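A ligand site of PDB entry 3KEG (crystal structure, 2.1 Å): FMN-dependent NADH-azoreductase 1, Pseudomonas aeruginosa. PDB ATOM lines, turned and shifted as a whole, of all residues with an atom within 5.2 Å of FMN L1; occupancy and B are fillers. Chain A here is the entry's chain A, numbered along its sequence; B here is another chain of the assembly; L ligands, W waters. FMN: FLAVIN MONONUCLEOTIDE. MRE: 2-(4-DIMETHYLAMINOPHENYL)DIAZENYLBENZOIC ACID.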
ATOM      1  N   SER A  10      -8.584  18.916  17.429  1.00  0.00           N
ATOM      2  CA  SER A  10      -9.706  18.256  18.090  1.00  0.00           C
ATOM      3  C   SER A  10     -10.885  19.217  18.227  1.00  0.00           C
ATOM      4  O   SER A  10     -10.698  20.371  18.601  1.00  0.00           O
ATOM      5  CB  SER A  10      -9.311  17.700  19.458  1.00  0.00           C
ATOM      6  OG  SER A  10     -10.442  17.127  20.098  1.00  0.00           O
ATOM      7  N   PRO A  11     -12.101  18.729  17.931  1.00  0.00           N
ATOM      8  CA  PRO A  11     -13.328  19.520  18.140  1.00  0.00           C
ATOM      9  C   PRO A  11     -13.648  19.668  19.623  1.00  0.00           C
ATOM     10  O   PRO A  11     -14.415  20.554  20.003  1.00  0.00           O
ATOM     11  CB  PRO A  11     -14.409  18.682  17.454  1.00  0.00           C
ATOM     12  CG  PRO A  11     -13.694  17.632  16.663  1.00  0.00           C
ATOM     13  CD  PRO A  11     -12.370  17.429  17.315  1.00  0.00           C
ATOM     14  N   ARG A  12     -13.069  18.798  20.445  1.00  0.00           N
ATOM     15  CA  ARG A  12     -13.344  18.803  21.872  1.00  0.00           C
ATOM     16  C   ARG A  12     -12.479  19.838  22.579  1.00  0.00           C
ATOM     17  O   ARG A  12     -11.391  20.166  22.126  1.00  0.00           O
ATOM     18  CB  ARG A  12     -13.092  17.422  22.479  1.00  0.00           C
ATOM     19  CG  ARG A  12     -13.894  16.309  21.812  1.00  0.00           C
ATOM     20  CD  ARG A  12     -14.119  15.121  22.730  1.00  0.00           C
ATOM     21  NE  ARG A  12     -12.899  14.361  22.986  1.00  0.00           N
ATOM     22  CZ  ARG A  12     -12.813  13.336  23.823  1.00  0.00           C
ATOM     23  NH1 ARG A  12     -11.657  12.697  23.981  1.00  0.00           N
ATOM     24  NH2 ARG A  12     -13.878  12.929  24.494  1.00  0.00           N
ATOM     25  N   ARG A  15     -12.068  18.090  27.219  1.00  0.00           N
ATOM     26  CA  ARG A  15     -11.970  16.623  27.115  1.00  0.00           C
ATOM     27  C   ARG A  15     -10.939  16.154  26.101  1.00  0.00           C
ATOM     28  O   ARG A  15     -10.662  14.959  26.018  1.00  0.00           O
ATOM     29  CB  ARG A  15     -13.324  16.003  26.727  1.00  0.00           C
ATOM     30  CG  ARG A  15     -14.349  15.946  27.842  1.00  0.00           C
ATOM     31  CD  ARG A  15     -13.781  15.552  29.184  1.00  0.00           C
ATOM     32  NE  ARG A  15     -14.125  16.585  30.155  1.00  0.00           N
ATOM     33  CZ  ARG A  15     -13.279  17.140  31.014  1.00  0.00           C
ATOM     34  NH1 ARG A  15     -12.001  16.766  31.055  1.00  0.00           N
ATOM     35  NH2 ARG A  15     -13.705  18.080  31.835  1.00  0.00           N
ATOM     36  N   SER A  16     -10.389  17.068  25.316  1.00  0.00           N
ATOM     37  CA  SER A  16      -9.432  16.680  24.289  1.00  0.00           C
ATOM     38  C   SER A  16      -8.109  16.271  24.926  1.00  0.00           C
ATOM     39  O   SER A  16      -7.449  17.087  25.567  1.00  0.00           O
ATOM     40  CB  SER A  16      -9.215  17.816  23.298  1.00  0.00           C
ATOM     41  OG  SER A  16      -8.169  17.509  22.404  1.00  0.00           O
ATOM     42  N   GLN A  17      -7.738  15.006  24.766  1.00  0.00           N
ATOM     43  CA  GLN A  17      -6.445  14.531  25.248  1.00  0.00           C
ATOM     44  C   GLN A  17      -5.298  15.100  24.411  1.00  0.00           C
ATOM     45  O   GLN A  17      -4.238  15.418  24.964  1.00  0.00           O
ATOM     46  CB  GLN A  17      -6.363  13.005  25.250  1.00  0.00           C
ATOM     47  CG  GLN A  17      -5.008  12.493  25.695  1.00  0.00           C
ATOM     48  CD  GLN A  17      -4.990  10.994  25.959  1.00  0.00           C
ATOM     49  OE1 GLN A  17      -5.428  10.202  25.131  1.00  0.00           O
ATOM     50  NE2 GLN A  17      -4.480  10.619  27.119  1.00  0.00           N
ATOM     51  N   SER A  18      -5.498  15.222  23.109  1.00  0.00           N
ATOM     52  CA  SER A  18      -4.448  15.752  22.230  1.00  0.00           C
ATOM     53  C   SER A  18      -4.219  17.249  22.461  1.00  0.00           C
ATOM     54  O   SER A  18      -3.083  17.724  22.441  1.00  0.00           O
ATOM     55  CB  SER A  18      -4.760  15.469  20.751  1.00  0.00           C
ATOM     56  OG  SER A  18      -5.901  16.163  20.306  1.00  0.00           O
ATOM     57  N   ARG A  19      -5.302  17.990  22.685  1.00  0.00           N
ATOM     58  CA  ARG A  19      -5.207  19.404  23.035  1.00  0.00           C
ATOM     59  C   ARG A  19      -4.500  19.567  24.369  1.00  0.00           C
ATOM     60  O   ARG A  19      -3.600  20.397  24.498  1.00  0.00           O
ATOM     61  CB  ARG A  19      -6.608  20.033  23.119  1.00  0.00           C
ATOM     62  CG  ARG A  19      -6.594  21.524  23.444  1.00  0.00           C
ATOM     63  CD  ARG A  19      -7.998  22.072  23.609  1.00  0.00           C
ATOM     64  NE  ARG A  19      -8.814  21.831  22.412  1.00  0.00           N
ATOM     65  CZ  ARG A  19      -8.834  22.622  21.353  1.00  0.00           C
ATOM     66  NH1 ARG A  19      -8.085  23.724  21.318  1.00  0.00           N
ATOM     67  NH2 ARG A  19      -9.612  22.318  20.326  1.00  0.00           N
ATOM     68  N   PRO A  96      -6.604  14.324  16.971  1.00  0.00           N
ATOM     69  CA  PRO A  96      -7.119  12.970  17.177  1.00  0.00           C
ATOM     70  C   PRO A  96      -6.934  12.150  15.906  1.00  0.00           C
ATOM     71  O   PRO A  96      -6.731  12.735  14.840  1.00  0.00           O
ATOM     72  CB  PRO A  96      -8.615  13.179  17.413  1.00  0.00           C
ATOM     73  CG  PRO A  96      -8.818  14.640  17.575  1.00  0.00           C
ATOM     74  CD  PRO A  96      -7.688  15.318  16.883  1.00  0.00           C
ATOM     75  N   MET A  97      -6.996  10.831  15.998  1.00  0.00           N
ATOM     76  CA  MET A  97      -7.175  10.025  14.806  1.00  0.00           C
ATOM     77  C   MET A  97      -8.673   9.820  14.617  1.00  0.00           C
ATOM     78  O   MET A  97      -9.335   9.202  15.444  1.00  0.00           O
ATOM     79  CB  MET A  97      -6.470   8.676  14.903  1.00  0.00           C
ATOM     80  CG  MET A  97      -6.903   7.708  13.814  1.00  0.00           C
ATOM     81  SD  MET A  97      -6.063   6.116  13.864  1.00  0.00           S
ATOM     82  CE  MET A  97      -4.489   6.540  13.111  1.00  0.00           C
ATOM     83  N   TYR A  98      -9.195  10.366  13.524  1.00  0.00           N
ATOM     84  CA  TYR A  98     -10.600  10.192  13.174  1.00  0.00           C
ATOM     85  C   TYR A  98     -10.704   9.288  11.943  1.00  0.00           C
ATOM     86  O   TYR A  98     -10.304   9.672  10.849  1.00  0.00           O
ATOM     87  CB  TYR A  98     -11.257  11.540  12.881  1.00  0.00           C
ATOM     88  CG  TYR A  98     -11.802  12.263  14.093  1.00  0.00           C
ATOM     89  CD1 TYR A  98     -11.479  11.850  15.380  1.00  0.00           C
ATOM     90  CD2 TYR A  98     -12.625  13.365  13.942  1.00  0.00           C
ATOM     91  CE1 TYR A  98     -11.986  12.522  16.482  1.00  0.00           C
ATOM     92  CE2 TYR A  98     -13.129  14.036  15.035  1.00  0.00           C
ATOM     93  CZ  TYR A  98     -12.807  13.609  16.301  1.00  0.00           C
ATOM     94  OH  TYR A  98     -13.312  14.281  17.393  1.00  0.00           O
ATOM     95  N   ASN A  99     -11.248   8.103  12.146  1.00  0.00           N
ATOM     96  CA  ASN A  99     -11.415   7.131  11.069  1.00  0.00           C
ATOM     97  C   ASN A  99     -10.151   6.973  10.242  1.00  0.00           C
ATOM     98  O   ASN A  99     -10.156   7.102   9.022  1.00  0.00           O
ATOM     99  CB  ASN A  99     -12.625   7.524  10.207  1.00  0.00           C
ATOM    100  CG  ASN A  99     -13.930   7.466  10.985  1.00  0.00           C
ATOM    101  OD1 ASN A  99     -14.310   6.427  11.502  1.00  0.00           O
ATOM    102  ND2 ASN A  99     -14.597   8.614  11.101  1.00  0.00           N
ATOM    103  N   PHE A 100      -9.048   6.697  10.947  1.00  0.00           N
ATOM    104  CA  PHE A 100      -7.757   6.370  10.348  1.00  0.00           C
ATOM    105  C   PHE A 100      -7.118   7.523   9.584  1.00  0.00           C
ATOM    106  O   PHE A 100      -6.188   7.328   8.809  1.00  0.00           O
ATOM    107  CB  PHE A 100      -7.904   5.138   9.439  1.00  0.00           C
ATOM    108  CG  PHE A 100      -8.678   4.022  10.076  1.00  0.00           C
ATOM    109  CD1 PHE A 100      -8.111   3.268  11.086  1.00  0.00           C
ATOM    110  CD2 PHE A 100      -9.972   3.745   9.679  1.00  0.00           C
ATOM    111  CE1 PHE A 100      -8.818   2.235  11.675  1.00  0.00           C
ATOM    112  CE2 PHE A 100     -10.691   2.721  10.264  1.00  0.00           C
ATOM    113  CZ  PHE A 100     -10.111   1.967  11.268  1.00  0.00           C
ATOM    114  N   SER A 145      -3.641  11.597  19.617  1.00  0.00           N
ATOM    115  CA  SER A 145      -4.209  10.569  20.481  1.00  0.00           C
ATOM    116  C   SER A 145      -5.152   9.692  19.667  1.00  0.00           C
ATOM    117  O   SER A 145      -5.798  10.150  18.728  1.00  0.00           O
ATOM    118  CB  SER A 145      -4.941  11.192  21.665  1.00  0.00           C
ATOM    119  OG  SER A 145      -5.958  12.076  21.227  1.00  0.00           O
ATOM    120  N   ARG A 146      -5.215   8.421  20.043  1.00  0.00           N
ATOM    121  CA  ARG A 146      -6.024   7.443  19.329  1.00  0.00           C
ATOM    122  C   ARG A 146      -6.770   6.584  20.338  1.00  0.00           C
ATOM    123  O   ARG A 146      -6.277   6.320  21.428  1.00  0.00           O
ATOM    124  CB  ARG A 146      -5.129   6.549  18.463  1.00  0.00           C
ATOM    125  CG  ARG A 146      -4.164   7.312  17.585  1.00  0.00           C
ATOM    126  CD  ARG A 146      -3.051   6.390  17.122  1.00  0.00           C
ATOM    127  NE  ARG A 146      -2.012   7.111  16.393  1.00  0.00           N
ATOM    128  CZ  ARG A 146      -0.718   6.812  16.443  1.00  0.00           C
ATOM    129  NH1 ARG A 146      -0.284   5.821  17.190  1.00  0.00           N
ATOM    130  NH2 ARG A 146       0.153   7.525  15.739  1.00  0.00           N
ATOM    131  N   GLY A 147      -7.971   6.150  19.968  1.00  0.00           N
ATOM    132  CA  GLY A 147      -8.754   5.275  20.815  1.00  0.00           C
ATOM    133  C   GLY A 147      -8.143   3.885  20.925  1.00  0.00           C
ATOM    134  O   GLY A 147      -8.161   3.275  21.997  1.00  0.00           O
ATOM    135  N   GLY A 148      -7.611   3.388  19.816  1.00  0.00           N
ATOM    136  CA  GLY A 148      -7.092   2.032  19.739  1.00  0.00           C
ATOM    137  C   GLY A 148      -5.588   1.941  19.913  1.00  0.00           C
ATOM    138  O   GLY A 148      -4.945   2.899  20.343  1.00  0.00           O
ATOM    139  N   HIS A 149      -5.032   0.787  19.565  1.00  0.00           N
ATOM    140  CA  HIS A 149      -3.601   0.526  19.759  1.00  0.00           C
ATOM    141  C   HIS A 149      -2.930   0.074  18.473  1.00  0.00           C
ATOM    142  O   HIS A 149      -3.593  -0.404  17.545  1.00  0.00           O
ATOM    143  CB  HIS A 149      -3.407  -0.568  20.812  1.00  0.00           C
ATOM    144  CG  HIS A 149      -3.899  -0.203  22.181  1.00  0.00           C
ATOM    145  ND1 HIS A 149      -5.159  -0.534  22.635  1.00  0.00           N
ATOM    146  CD2 HIS A 149      -3.297   0.461  23.188  1.00  0.00           C
ATOM    147  CE1 HIS A 149      -5.306  -0.091  23.868  1.00  0.00           C
ATOM    148  NE2 HIS A 149      -4.187   0.524  24.224  1.00  0.00           N
ATOM    149  N   PHE A 151      -1.018   1.675  16.085  1.00  0.00           N
ATOM    150  CA  PHE A 151      -0.991   2.470  14.862  1.00  0.00           C
ATOM    151  C   PHE A 151       0.370   3.118  14.630  1.00  0.00           C
ATOM    152  O   PHE A 151       0.617   3.713  13.590  1.00  0.00           O
ATOM    153  CB  PHE A 151      -2.090   3.540  14.901  1.00  0.00           C
ATOM    154  CG  PHE A 151      -3.477   2.979  14.762  1.00  0.00           C
ATOM    155  CD1 PHE A 151      -3.963   2.585  13.529  1.00  0.00           C
ATOM    156  CD2 PHE A 151      -4.302   2.837  15.872  1.00  0.00           C
ATOM    157  CE1 PHE A 151      -5.241   2.070  13.394  1.00  0.00           C
ATOM    158  CE2 PHE A 151      -5.581   2.322  15.737  1.00  0.00           C
ATOM    159  CZ  PHE A 151      -6.046   1.940  14.500  1.00  0.00           C
ATOM    160  N   VAL B  51     -17.230  17.037  12.151  1.00  0.00           N
ATOM    161  CA  VAL B  51     -17.625  16.455  13.425  1.00  0.00           C
ATOM    162  C   VAL B  51     -17.329  17.432  14.560  1.00  0.00           C
ATOM    163  O   VAL B  51     -16.206  17.897  14.706  1.00  0.00           O
ATOM    164  CB  VAL B  51     -16.894  15.131  13.679  1.00  0.00           C
ATOM    165  CG1 VAL B  51     -16.911  14.781  15.167  1.00  0.00           C
ATOM    166  CG2 VAL B  51     -17.520  14.010  12.853  1.00  0.00           C
ATOM    167  N   PHE B  55     -21.471  16.287  18.293  1.00  0.00           N
ATOM    168  CA  PHE B  55     -21.608  15.062  17.505  1.00  0.00           C
ATOM    169  C   PHE B  55     -21.014  13.880  18.263  1.00  0.00           C
ATOM    170  O   PHE B  55     -21.635  12.821  18.341  1.00  0.00           O
ATOM    171  CB  PHE B  55     -20.910  15.205  16.146  1.00  0.00           C
ATOM    172  CG  PHE B  55     -20.960  13.955  15.306  1.00  0.00           C
ATOM    173  CD1 PHE B  55     -21.937  13.796  14.343  1.00  0.00           C
ATOM    174  CD2 PHE B  55     -20.037  12.943  15.497  1.00  0.00           C
ATOM    175  CE1 PHE B  55     -21.985  12.646  13.570  1.00  0.00           C
ATOM    176  CE2 PHE B  55     -20.076  11.795  14.727  1.00  0.00           C
ATOM    177  CZ  PHE B  55     -21.055  11.646  13.763  1.00  0.00           C
ATOM    178  N   VAL B  56     -19.818  14.062  18.803  1.00  0.00           N
ATOM    179  CA  VAL B  56     -19.137  12.989  19.530  1.00  0.00           C
ATOM    180  C   VAL B  56     -19.936  12.549  20.750  1.00  0.00           C
ATOM    181  O   VAL B  56     -20.092  11.363  21.009  1.00  0.00           O
ATOM    182  CB  VAL B  56     -17.723  13.420  19.967  1.00  0.00           C
ATOM    183  CG1 VAL B  56     -17.020  12.280  20.697  1.00  0.00           C
ATOM    184  CG2 VAL B  56     -16.903  13.844  18.756  1.00  0.00           C
ATOM    185  N   PHE B  60     -21.698   8.676  20.569  1.00  0.00           N
ATOM    186  CA  PHE B  60     -21.118   7.673  21.456  1.00  0.00           C
ATOM    187  C   PHE B  60     -21.816   7.652  22.816  1.00  0.00           C
ATOM    188  O   PHE B  60     -21.287   7.112  23.794  1.00  0.00           O
ATOM    189  CB  PHE B  60     -19.626   7.927  21.638  1.00  0.00           C
ATOM    190  CG  PHE B  60     -18.834   7.789  20.370  1.00  0.00           C
ATOM    191  CD1 PHE B  60     -18.227   6.586  20.055  1.00  0.00           C
ATOM    192  CD2 PHE B  60     -18.683   8.853  19.510  1.00  0.00           C
ATOM    193  CE1 PHE B  60     -17.493   6.445  18.894  1.00  0.00           C
ATOM    194  CE2 PHE B  60     -17.952   8.732  18.346  1.00  0.00           C
ATOM    195  CZ  PHE B  60     -17.357   7.527  18.037  1.00  0.00           C
ATOM    196  N   ASP B 111     -16.553  10.902   8.199  1.00  0.00           N
ATOM    197  CA  ASP B 111     -16.706  11.116   9.631  1.00  0.00           C
ATOM    198  C   ASP B 111     -18.174  11.123  10.076  1.00  0.00           C
ATOM    199  O   ASP B 111     -18.472  10.823  11.232  1.00  0.00           O
ATOM    200  CB  ASP B 111     -16.027  12.424  10.054  1.00  0.00           C
ATOM    201  CG  ASP B 111     -14.507  12.323  10.064  1.00  0.00           C
ATOM    202  OD1 ASP B 111     -13.987  11.201   9.988  1.00  0.00           O
ATOM    203  OD2 ASP B 111     -13.859  13.379  10.156  1.00  0.00           O
HETATM  204  N1  FMN L   1      -9.491   5.868  17.428  1.00  0.00           N
HETATM  205  C2  FMN L   1      -8.701   5.008  16.691  1.00  0.00           C
HETATM  206  O2  FMN L   1      -7.824   4.343  17.230  1.00  0.00           O
HETATM  207  N3  FMN L   1      -8.879   4.871  15.335  1.00  0.00           N
HETATM  208  C4  FMN L   1      -9.858   5.613  14.709  1.00  0.00           C
HETATM  209  O4  FMN L   1     -10.014   5.499  13.497  1.00  0.00           O
HETATM  210  C4A FMN L   1     -10.658   6.481  15.441  1.00  0.00           C
HETATM  211  N5  FMN L   1     -11.629   7.211  14.798  1.00  0.00           N
HETATM  212  C5A FMN L   1     -12.423   8.077  15.511  1.00  0.00           C
HETATM  213  C6  FMN L   1     -13.413   8.814  14.861  1.00  0.00           C
HETATM  214  C7  FMN L   1     -14.228   9.696  15.565  1.00  0.00           C
HETATM  215  C7M FMN L   1     -15.279  10.463  14.825  1.00  0.00           C
HETATM  216  C8  FMN L   1     -14.056   9.843  16.929  1.00  0.00           C
HETATM  217  C8M FMN L   1     -14.947  10.766  17.709  1.00  0.00           C
HETATM  218  C9  FMN L   1     -13.073   9.095  17.578  1.00  0.00           C
HETATM  219  C9A FMN L   1     -12.249   8.214  16.877  1.00  0.00           C
HETATM  220  N10 FMN L   1     -11.276   7.474  17.522  1.00  0.00           N
HETATM  221  C10 FMN L   1     -10.475   6.620  16.810  1.00  0.00           C
HETATM  222  C1' FMN L   1     -11.078   7.629  18.991  1.00  0.00           C
HETATM  223  C2' FMN L   1     -10.277   8.922  19.108  1.00  0.00           C
HETATM  224  O2' FMN L   1      -9.138   8.790  18.286  1.00  0.00           O
HETATM  225  C3' FMN L   1      -9.883   9.241  20.549  1.00  0.00           C
HETATM  226  O3' FMN L   1     -11.044   9.466  21.323  1.00  0.00           O
HETATM  227  C4' FMN L   1      -8.949  10.448  20.573  1.00  0.00           C
HETATM  228  O4' FMN L   1      -8.264  10.504  21.812  1.00  0.00           O
HETATM  229  C5' FMN L   1      -9.681  11.759  20.298  1.00  0.00           C
HETATM  230  O5' FMN L   1      -8.773  12.816  20.443  1.00  0.00           O
HETATM  231  P   FMN L   1      -9.114  13.991  21.487  1.00  0.00           P
HETATM  232  O1P FMN L   1      -9.119  13.373  22.864  1.00  0.00           O
HETATM  233  O2P FMN L   1     -10.468  14.569  21.155  1.00  0.00           O
HETATM  234  O3P FMN L   1      -8.054  15.058  21.408  1.00  0.00           O
HETATM  235  C1  MRE L   2     -12.563   3.960  16.288  1.00  0.00           C
HETATM  236  C2  MRE L   2     -13.311   4.778  17.204  1.00  0.00           C
HETATM  237  C3  MRE L   2     -14.350   5.608  16.612  1.00  0.00           C
HETATM  238  C4  MRE L   2     -14.614   5.582  15.108  1.00  0.00           C
HETATM  239  C5  MRE L   2     -13.887   4.779  14.247  1.00  0.00           C
HETATM  240  C6  MRE L   2     -12.813   3.924  14.842  1.00  0.00           C
HETATM  241  C1' MRE L   2     -10.217   1.450  15.890  1.00  0.00           C
HETATM  242  C2' MRE L   2      -9.944   0.844  14.685  1.00  0.00           C
HETATM  243  C3' MRE L   2      -9.029  -0.252  14.635  1.00  0.00           C
HETATM  244  C4' MRE L   2      -8.413  -0.727  15.852  1.00  0.00           C
HETATM  245  C5' MRE L   2      -8.692  -0.107  17.096  1.00  0.00           C
HETATM  246  C6' MRE L   2      -9.604   0.998  17.136  1.00  0.00           C
HETATM  247  C   MRE L   2     -12.951   4.709  18.666  1.00  0.00           C
HETATM  248  CHX MRE L   2      -6.869  -1.972  14.388  1.00  0.00           C
HETATM  249  CHZ MRE L   2      -7.163  -2.702  16.802  1.00  0.00           C
HETATM  250  N1  MRE L   2     -11.491   3.160  16.771  1.00  0.00           N
HETATM  251  N1' MRE L   2     -11.120   2.547  15.784  1.00  0.00           N
HETATM  252  OXT MRE L   2     -13.524   5.394  19.551  1.00  0.00           O
HETATM  253  O   MRE L   2     -12.031   3.961  19.004  1.00  0.00           O
HETATM  254  N10 MRE L   2      -7.453  -1.840  15.712  1.00  0.00           N
HETATM  255  O   HOH W   1     -17.348   8.871  12.775  1.00  0.00           O
HETATM  256  O   HOH W   2     -12.510  13.440  19.865  1.00  0.00           O
HETATM  257  O   HOH W   3     -13.195  10.960  21.015  1.00  0.00           O
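Water W2 lies within hydrogen-bond range of O2P of FMN L1 (2.7 Å), OH of Tyr 98 (2.7 Å) and NE of Arg 12 (3.3 Å).
Water W1 bridges the backbone carbonyl oxygen (O) of Asp 111 of chain B and the side-chain amide nitrogen (ND2) of Asn 99.
N1' of MRE L2 is in hydrogen-bond range of N3 of FMN L1 (3.3 Å).
OG of Ser 10 sits at hydrogen-bond distance from N of Arg 12, 3.1 Å away.
N of Arg 19 is in hydrogen-bond range of OG of Ser 16.
The side-chain hydroxyl (OG) of Ser 16 is in hydrogen-bond range of the side-chain hydroxyl (OG) of Ser 18 (3.4 Å).
The side-chain hydroxyl (OG) of Ser 16 lies close to the side-chain hydroxyl (OG) of Ser 10 (3.3 Å).
The guanidinium group (NH1) of Arg 12 lies within hydrogen-bond range of the backbone carbonyl oxygen (O) of Arg 15, 3.2 Å away.
OD1 of Asp 111 of chain B sits at hydrogen-bond distance from ND2 of Asn 99, 2.9 Å away.
The guanidinium group of Arg 19 lies within hydrogen-bond range of the backbone carbonyl oxygen of Arg 12 (3.1 Å).
The backbone carbonyl oxygen (O) of Ser 10 is in hydrogen-bond range of the guanidinium group (NH2) of Arg 19, at 2.8 Å.
N1 of FMN L1 sits at hydrogen-bond distance from N of Gly 147, 3.0 Å away.
The side-chain hydroxyl of Ser 16 is in hydrogen-bond range of an oxygen (O3P) of FMN L1, at 2.6 Å.
The backbone NH (N) of Gln 17 is in hydrogen-bond range of an oxygen (O1P) of FMN L1 (2.9 Å).
O2P of FMN L1 is in hydrogen-bond range of OG of Ser 10.
The backbone NH of Asn 99 lies within hydrogen-bond range of a nitrogen (N5) of FMN L1.
N of Ser 18 sits at hydrogen-bond distance from O3P of FMN L1 (3.1 Å).
The side-chain hydroxyl (OG) of Ser 18 is in hydrogen-bond range of an oxygen (O3P) of FMN L1 (2.7 Å).
An oxygen (O1P) of FMN L1 is in salt-bridge range of the guanidinium group (NH1) of Arg 12 (2.9 Å).
SD of Met 97 sits at hydrogen-bond distance from N3 of FMN L1 (3.4 Å).
An oxygen (O2) of FMN L1 is in hydrogen-bond range of the backbone NH of Gly 148.
OG of Ser 145 lies within hydrogen-bond range of O4' of FMN L1.
The backbone carbonyl oxygen (O) of Met 97 sits at hydrogen-bond distance from an oxygen (O2') of FMN L1, 2.9 Å away.
N of Phe 100 is in hydrogen-bond range of O4 of FMN L1, at 3.0 Å.
Merely in contact with FMN L1: Pro 96, Phe 151, Tyr 98, Arg 146, Phe 60 of chain B, Val 56 of chain B and Arg 15.
Hydrophobic or aromatic side chains that line FMN L1: Pro 96, Met 97, Tyr 98, Phe 100, Phe 151, Val 56 of chain B and Phe 60 of chain B.
Of the 24 residues printed, 18 come within 4 Å of FMN L1.
The nearest printed residue that does not touch FMN L1 is Arg 19 (4.2 Å).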
